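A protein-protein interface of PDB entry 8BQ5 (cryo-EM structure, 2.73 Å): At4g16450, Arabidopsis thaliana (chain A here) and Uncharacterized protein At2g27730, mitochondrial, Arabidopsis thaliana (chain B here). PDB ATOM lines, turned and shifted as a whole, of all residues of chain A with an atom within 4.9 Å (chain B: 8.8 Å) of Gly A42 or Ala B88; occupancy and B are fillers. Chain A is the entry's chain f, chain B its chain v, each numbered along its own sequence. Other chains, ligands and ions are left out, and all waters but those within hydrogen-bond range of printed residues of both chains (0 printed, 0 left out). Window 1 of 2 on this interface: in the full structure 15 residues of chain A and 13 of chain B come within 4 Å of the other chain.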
ATOM      1  N   SER A  38      17.745 -21.256 -21.290  1.00  0.00           N
ATOM      2  CA  SER A  38      16.709 -21.984 -20.514  1.00  0.00           C
ATOM      3  C   SER A  38      16.717 -21.549 -19.045  1.00  0.00           C
ATOM      4  O   SER A  38      15.626 -21.390 -18.487  1.00  0.00           O
ATOM      5  CB  SER A  38      16.914 -23.457 -20.652  1.00  0.00           C
ATOM      6  OG  SER A  38      16.868 -23.845 -22.014  1.00  0.00           O
ATOM      7  N   THR A  39      17.900 -21.356 -18.453  1.00  0.00           N
ATOM      8  CA  THR A  39      17.995 -20.893 -17.048  1.00  0.00           C
ATOM      9  C   THR A  39      17.325 -19.526 -16.917  1.00  0.00           C
ATOM     10  O   THR A  39      16.511 -19.371 -15.998  1.00  0.00           O
ATOM     11  CB  THR A  39      19.444 -20.822 -16.562  1.00  0.00           C
ATOM     12  OG1 THR A  39      20.076 -22.073 -16.826  1.00  0.00           O
ATOM     13  CG2 THR A  39      19.561 -20.491 -15.091  1.00  0.00           C
ATOM     14  N   ILE A  40      17.645 -18.587 -17.811  1.00  0.00           N
ATOM     15  CA  ILE A  40      17.096 -17.201 -17.705  1.00  0.00           C
ATOM     16  C   ILE A  40      15.577 -17.254 -17.911  1.00  0.00           C
ATOM     17  O   ILE A  40      14.867 -16.599 -17.144  1.00  0.00           O
ATOM     18  CB  ILE A  40      17.815 -16.241 -18.677  1.00  0.00           C
ATOM     19  CG1 ILE A  40      19.303 -16.115 -18.336  1.00  0.00           C
ATOM     20  CG2 ILE A  40      17.139 -14.880 -18.718  1.00  0.00           C
ATOM     21  CD1 ILE A  40      20.103 -15.310 -19.330  1.00  0.00           C
ATOM     22  N   THR A  41      15.108 -18.031 -18.885  1.00  0.00           N
ATOM     23  CA  THR A  41      13.646 -18.169 -19.131  1.00  0.00           C
ATOM     24  C   THR A  41      12.961 -18.812 -17.911  1.00  0.00           C
ATOM     25  O   THR A  41      11.896 -18.308 -17.532  1.00  0.00           O
ATOM     26  CB  THR A  41      13.359 -18.868 -20.463  1.00  0.00           C
ATOM     27  OG1 THR A  41      14.116 -18.200 -21.472  1.00  0.00           O
ATOM     28  CG2 THR A  41      11.892 -18.857 -20.826  1.00  0.00           C
ATOM     29  N   GLY A  42      13.561 -19.837 -17.296  1.00  0.00           N
ATOM     30  CA  GLY A  42      12.933 -20.486 -16.158  1.00  0.00           C
ATOM     31  C   GLY A  42      12.897 -19.604 -14.929  1.00  0.00           C
ATOM     32  O   GLY A  42      11.881 -19.541 -14.230  1.00  0.00           O
ATOM     33  N   ILE A  43      13.999 -18.904 -14.649  1.00  0.00           N
ATOM     34  CA  ILE A  43      14.017 -17.972 -13.527  1.00  0.00           C
ATOM     35  C   ILE A  43      12.972 -16.885 -13.726  1.00  0.00           C
ATOM     36  O   ILE A  43      12.261 -16.507 -12.786  1.00  0.00           O
ATOM     37  CB  ILE A  43      15.424 -17.374 -13.346  1.00  0.00           C
ATOM     38  CG1 ILE A  43      16.377 -18.413 -12.755  1.00  0.00           C
ATOM     39  CG2 ILE A  43      15.371 -16.133 -12.473  1.00  0.00           C
ATOM     40  CD1 ILE A  43      17.830 -18.018 -12.848  1.00  0.00           C
ATOM     41  N   SER A  44      12.865 -16.357 -14.948  1.00  0.00           N
ATOM     42  CA  SER A  44      11.895 -15.298 -15.201  1.00  0.00           C
ATOM     43  C   SER A  44      10.464 -15.791 -15.015  1.00  0.00           C
ATOM     44  O   SER A  44       9.635 -15.088 -14.424  1.00  0.00           O
ATOM     45  CB  SER A  44      12.103 -14.735 -16.601  1.00  0.00           C
ATOM     46  OG  SER A  44      13.415 -14.224 -16.742  1.00  0.00           O
ATOM     47  N   VAL A  45      10.155 -16.995 -15.503  1.00  0.00           N
ATOM     48  CA  VAL A  45       8.814 -17.544 -15.305  1.00  0.00           C
ATOM     49  C   VAL A  45       8.535 -17.749 -13.820  1.00  0.00           C
ATOM     50  O   VAL A  45       7.431 -17.470 -13.334  1.00  0.00           O
ATOM     51  CB  VAL A  45       8.641 -18.850 -16.104  1.00  0.00           C
ATOM     52  CG1 VAL A  45       7.302 -19.489 -15.789  1.00  0.00           C
ATOM     53  CG2 VAL A  45       8.744 -18.579 -17.589  1.00  0.00           C
ATOM     54  N   THR A  46       9.530 -18.240 -13.074  1.00  0.00           N
ATOM     55  CA  THR A  46       9.354 -18.442 -11.640  1.00  0.00           C
ATOM     56  C   THR A  46       9.066 -17.127 -10.924  1.00  0.00           C
ATOM     57  O   THR A  46       8.163 -17.054 -10.079  1.00  0.00           O
ATOM     58  CB  THR A  46      10.598 -19.109 -11.053  1.00  0.00           C
ATOM     59  OG1 THR A  46      10.653 -20.477 -11.474  1.00  0.00           O
ATOM     60  CG2 THR A  46      10.579 -19.050  -9.532  1.00  0.00           C
ATOM     61  N   ASN B  81      -1.436 -23.926 -13.790  1.00  0.00           N
ATOM     62  CA  ASN B  81      -0.463 -22.841 -13.695  1.00  0.00           C
ATOM     63  C   ASN B  81       0.612 -23.162 -12.666  1.00  0.00           C
ATOM     64  O   ASN B  81       1.799 -22.902 -12.892  1.00  0.00           O
ATOM     65  CB  ASN B  81      -1.165 -21.532 -13.340  1.00  0.00           C
ATOM     66  CG  ASN B  81      -1.858 -20.901 -14.527  1.00  0.00           C
ATOM     67  OD1 ASN B  81      -1.601 -21.256 -15.675  1.00  0.00           O
ATOM     68  ND2 ASN B  81      -2.742 -19.952 -14.253  1.00  0.00           N
ATOM     69  N   ARG B  82       0.211 -23.730 -11.528  1.00  0.00           N
ATOM     70  CA  ARG B  82       1.183 -24.123 -10.515  1.00  0.00           C
ATOM     71  C   ARG B  82       2.102 -25.222 -11.033  1.00  0.00           C
ATOM     72  O   ARG B  82       3.300 -25.224 -10.742  1.00  0.00           O
ATOM     73  CB  ARG B  82       0.462 -24.570  -9.243  1.00  0.00           C
ATOM     74  CG  ARG B  82       1.387 -24.832  -8.068  1.00  0.00           C
ATOM     75  CD  ARG B  82       0.612 -25.292  -6.846  1.00  0.00           C
ATOM     76  NE  ARG B  82      -0.015 -26.593  -7.049  1.00  0.00           N
ATOM     77  CZ  ARG B  82      -1.285 -26.862  -6.784  1.00  0.00           C
ATOM     78  NH1 ARG B  82      -2.105 -25.936  -6.316  1.00  0.00           N
ATOM     79  NH2 ARG B  82      -1.745 -28.091  -6.997  1.00  0.00           N
ATOM     80  N   ASN B  83       1.557 -26.167 -11.802  1.00  0.00           N
ATOM     81  CA  ASN B  83       2.389 -27.212 -12.393  1.00  0.00           C
ATOM     82  C   ASN B  83       3.409 -26.626 -13.361  1.00  0.00           C
ATOM     83  O   ASN B  83       4.583 -27.018 -13.354  1.00  0.00           O
ATOM     84  CB  ASN B  83       1.507 -28.235 -13.106  1.00  0.00           C
ATOM     85  CG  ASN B  83       0.534 -28.909 -12.170  1.00  0.00           C
ATOM     86  OD1 ASN B  83       0.639 -28.779 -10.950  1.00  0.00           O
ATOM     87  ND2 ASN B  83      -0.426 -29.633 -12.731  1.00  0.00           N
ATOM     88  N   TYR B  84       2.975 -25.684 -14.201  1.00  0.00           N
ATOM     89  CA  TYR B  84       3.899 -25.022 -15.115  1.00  0.00           C
ATOM     90  C   TYR B  84       4.985 -24.278 -14.353  1.00  0.00           C
ATOM     91  O   TYR B  84       6.156 -24.306 -14.743  1.00  0.00           O
ATOM     92  CB  TYR B  84       3.145 -24.057 -16.026  1.00  0.00           C
ATOM     93  CG  TYR B  84       2.061 -24.684 -16.865  1.00  0.00           C
ATOM     94  CD1 TYR B  84       2.052 -26.046 -17.135  1.00  0.00           C
ATOM     95  CD2 TYR B  84       1.042 -23.907 -17.390  1.00  0.00           C
ATOM     96  CE1 TYR B  84       1.058 -26.610 -17.907  1.00  0.00           C
ATOM     97  CE2 TYR B  84       0.052 -24.458 -18.159  1.00  0.00           C
ATOM     98  CZ  TYR B  84       0.061 -25.805 -18.414  1.00  0.00           C
ATOM     99  OH  TYR B  84      -0.937 -26.331 -19.189  1.00  0.00           O
ATOM    100  N   ALA B  85       4.611 -23.597 -13.270  1.00  0.00           N
ATOM    101  CA  ALA B  85       5.600 -22.885 -12.467  1.00  0.00           C
ATOM    102  C   ALA B  85       6.580 -23.849 -11.809  1.00  0.00           C
ATOM    103  O   ALA B  85       7.771 -23.546 -11.680  1.00  0.00           O
ATOM    104  CB  ALA B  85       4.901 -22.031 -11.414  1.00  0.00           C
ATOM    105  N   VAL B  86       6.090 -25.008 -11.367  1.00  0.00           N
ATOM    106  CA  VAL B  86       6.971 -26.018 -10.786  1.00  0.00           C
ATOM    107  C   VAL B  86       7.972 -26.500 -11.827  1.00  0.00           C
ATOM    108  O   VAL B  86       9.172 -26.631 -11.547  1.00  0.00           O
ATOM    109  CB  VAL B  86       6.136 -27.177 -10.210  1.00  0.00           C
ATOM    110  CG1 VAL B  86       7.001 -28.401  -9.975  1.00  0.00           C
ATOM    111  CG2 VAL B  86       5.460 -26.746  -8.919  1.00  0.00           C
ATOM    112  N   VAL B  87       7.497 -26.748 -13.048  1.00  0.00           N
ATOM    113  CA  VAL B  87       8.391 -27.160 -14.127  1.00  0.00           C
ATOM    114  C   VAL B  87       9.407 -26.065 -14.430  1.00  0.00           C
ATOM    115  O   VAL B  87      10.581 -26.346 -14.689  1.00  0.00           O
ATOM    116  CB  VAL B  87       7.576 -27.545 -15.375  1.00  0.00           C
ATOM    117  CG1 VAL B  87       8.488 -27.730 -16.579  1.00  0.00           C
ATOM    118  CG2 VAL B  87       6.788 -28.808 -15.107  1.00  0.00           C
ATOM    119  N   ALA B  88       8.973 -24.803 -14.408  1.00  0.00           N
ATOM    120  CA  ALA B  88       9.889 -23.694 -14.659  1.00  0.00           C
ATOM    121  C   ALA B  88      10.970 -23.605 -13.588  1.00  0.00           C
ATOM    122  O   ALA B  88      12.141 -23.364 -13.898  1.00  0.00           O
ATOM    123  CB  ALA B  88       9.117 -22.380 -14.740  1.00  0.00           C
ATOM    124  N   GLY B  89      10.594 -23.773 -12.321  1.00  0.00           N
ATOM    125  CA  GLY B  89      11.592 -23.775 -11.262  1.00  0.00           C
ATOM    126  C   GLY B  89      12.565 -24.932 -11.391  1.00  0.00           C
ATOM    127  O   GLY B  89      13.770 -24.779 -11.166  1.00  0.00           O
ATOM    128  N   VAL B  90      12.055 -26.105 -11.768  1.00  0.00           N
ATOM    129  CA  VAL B  90      12.922 -27.259 -11.975  1.00  0.00           C
ATOM    130  C   VAL B  90      13.887 -27.002 -13.124  1.00  0.00           C
ATOM    131  O   VAL B  90      15.077 -27.322 -13.037  1.00  0.00           O
ATOM    132  CB  VAL B  90      12.074 -28.522 -12.211  1.00  0.00           C
ATOM    133  CG1 VAL B  90      12.930 -29.654 -12.750  1.00  0.00           C
ATOM    134  CG2 VAL B  90      11.395 -28.930 -10.924  1.00  0.00           C
ATOM    135  N   VAL B  91      13.387 -26.428 -14.220  1.00  0.00           N
ATOM    136  CA  VAL B  91      14.239 -26.112 -15.362  1.00  0.00           C
ATOM    137  C   VAL B  91      15.289 -25.083 -14.971  1.00  0.00           C
ATOM    138  O   VAL B  91      16.449 -25.183 -15.375  1.00  0.00           O
ATOM    139  CB  VAL B  91      13.388 -25.634 -16.554  1.00  0.00           C
ATOM    140  CG1 VAL B  91      14.264 -24.997 -17.622  1.00  0.00           C
ATOM    141  CG2 VAL B  91      12.615 -26.800 -17.147  1.00  0.00           C
ATOM    142  N   ALA B  92      14.908 -24.092 -14.165  1.00  0.00           N
ATOM    143  CA  ALA B  92      15.877 -23.107 -13.696  1.00  0.00           C
ATOM    144  C   ALA B  92      16.986 -23.771 -12.892  1.00  0.00           C
ATOM    145  O   ALA B  92      18.174 -23.506 -13.115  1.00  0.00           O
ATOM    146  CB  ALA B  92      15.175 -22.035 -12.862  1.00  0.00           C
ATOM    147  N   ILE B  93      16.620 -24.662 -11.967  1.00  0.00           N
ATOM    148  CA  ILE B  93      17.619 -25.307 -11.116  1.00  0.00           C
ATOM    149  C   ILE B  93      18.539 -26.198 -11.947  1.00  0.00           C
ATOM    150  O   ILE B  93      19.774 -26.133 -11.835  1.00  0.00           O
ATOM    151  CB  ILE B  93      16.928 -26.095  -9.987  1.00  0.00           C
ATOM    152  CG1 ILE B  93      16.487 -25.145  -8.873  1.00  0.00           C
ATOM    153  CG2 ILE B  93      17.849 -27.166  -9.426  1.00  0.00           C
ATOM    154  CD1 ILE B  93      15.191 -25.545  -8.209  1.00  0.00           C
ATOM    155  N   VAL B  94      17.952 -27.038 -12.804  1.00  0.00           N
ATOM    156  CA  VAL B  94      18.744 -27.964 -13.607  1.00  0.00           C
ATOM    157  C   VAL B  94      19.624 -27.204 -14.591  1.00  0.00           C
ATOM    158  O   VAL B  94      20.779 -27.577 -14.828  1.00  0.00           O
ATOM    159  CB  VAL B  94      17.822 -28.968 -14.323  1.00  0.00           C
ATOM    160  CG1 VAL B  94      18.632 -29.902 -15.202  1.00  0.00           C
ATOM    161  CG2 VAL B  94      17.018 -29.763 -13.309  1.00  0.00           C
ATOM    162  N   GLY B  95      19.097 -26.128 -15.176  1.00  0.00           N
ATOM    163  CA  GLY B  95      19.892 -25.315 -16.073  1.00  0.00           C
ATOM    164  C   GLY B  95      21.036 -24.618 -15.369  1.00  0.00           C
ATOM    165  O   GLY B  95      22.120 -24.483 -15.932  1.00  0.00           O
ATOM    166  N   SER B  96      20.815 -24.156 -14.135  1.00  0.00           N
ATOM    167  CA  SER B  96      21.912 -23.567 -13.373  1.00  0.00           C
ATOM    168  C   SER B  96      23.000 -24.598 -13.102  1.00  0.00           C
ATOM    169  O   SER B  96      24.198 -24.302 -13.224  1.00  0.00           O
ATOM    170  CB  SER B  96      21.392 -22.981 -12.061  1.00  0.00           C
ATOM    171  OG  SER B  96      20.542 -21.872 -12.291  1.00  0.00           O
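Printed residues of chain B within 4 Å of Ser A38: Val B91 (3.95 Å). Thr A41 touches none of the printed residues of chain B. Of chain B, only Ala B88 and Ala B92 come within 4 Å of Gly A42. Of the printed residues of chain B, Thr A46 touches Ala B88 and Gly B89. Ala B85 touches none of the printed residues of chain A. Val B86 touches none of the printed residues of chain A. Ala B88 touches just these residues of chain A: Gly A42, Val A45 and Thr A46. Of the printed residues of chain A, Gly B89 touches Thr A46 (3.4 Å). Of the printed residues of chain A, Ala B92 touches Thr A39 (3.9 Å), Gly A42 (3.9 Å) and Ile A43 (3.8 Å). The nearest residue of chain B that does not touch Gly A42 is Gly B89 (4.8 Å). The nearest printed residue of chain A that does not touch Ala B88 is Ile A43 (4.9 Å).
Among the printed residues, merely in contact across the chains: Val A45 with Ala B88, Gly A42 with Ala B88, Thr A46 with Ala B88, Ile A43 with Ala B92, Thr A39 with Ala B92, Gly A42 with Ala B92 and Ser A38 with Val B91.
Of the 9 printed residues of chain A, 6 touch a printed residue of chain B. Printed residues of chain A that touch a printed residue of chain B: Ser A38, Thr A39, Gly A42, Ile A43, Val A45 and Thr A46. Hydrophobic or aromatic side chains of chain A that line the printed part of chain B: Ile A43 and Val A45. Among the printed residues, no Asp or Glu carboxylate lies within 4 Å of a Lys or Arg side-chain nitrogen of the other chain.
O of Gly A42 is in hydrogen-bond range of OG1 of Thr A46 (3.2 Å). The side-chain hydroxyl of Ser B96 lies within hydrogen-bond range of the backbone carbonyl oxygen of Ala B92 (3.0 Å).
The side-chain hydroxyl (OG1) of Thr A39 lies close to the backbone carbonyl oxygen (O) of Gly B95 (3.3 Å). N of Ser B96 sits at hydrogen-bond distance from OG1 of Thr A39 (3.5 Å). The side-chain hydroxyl of Thr A46 sits at hydrogen-bond distance from the backbone NH of Gly B89, 3.4 Å away.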
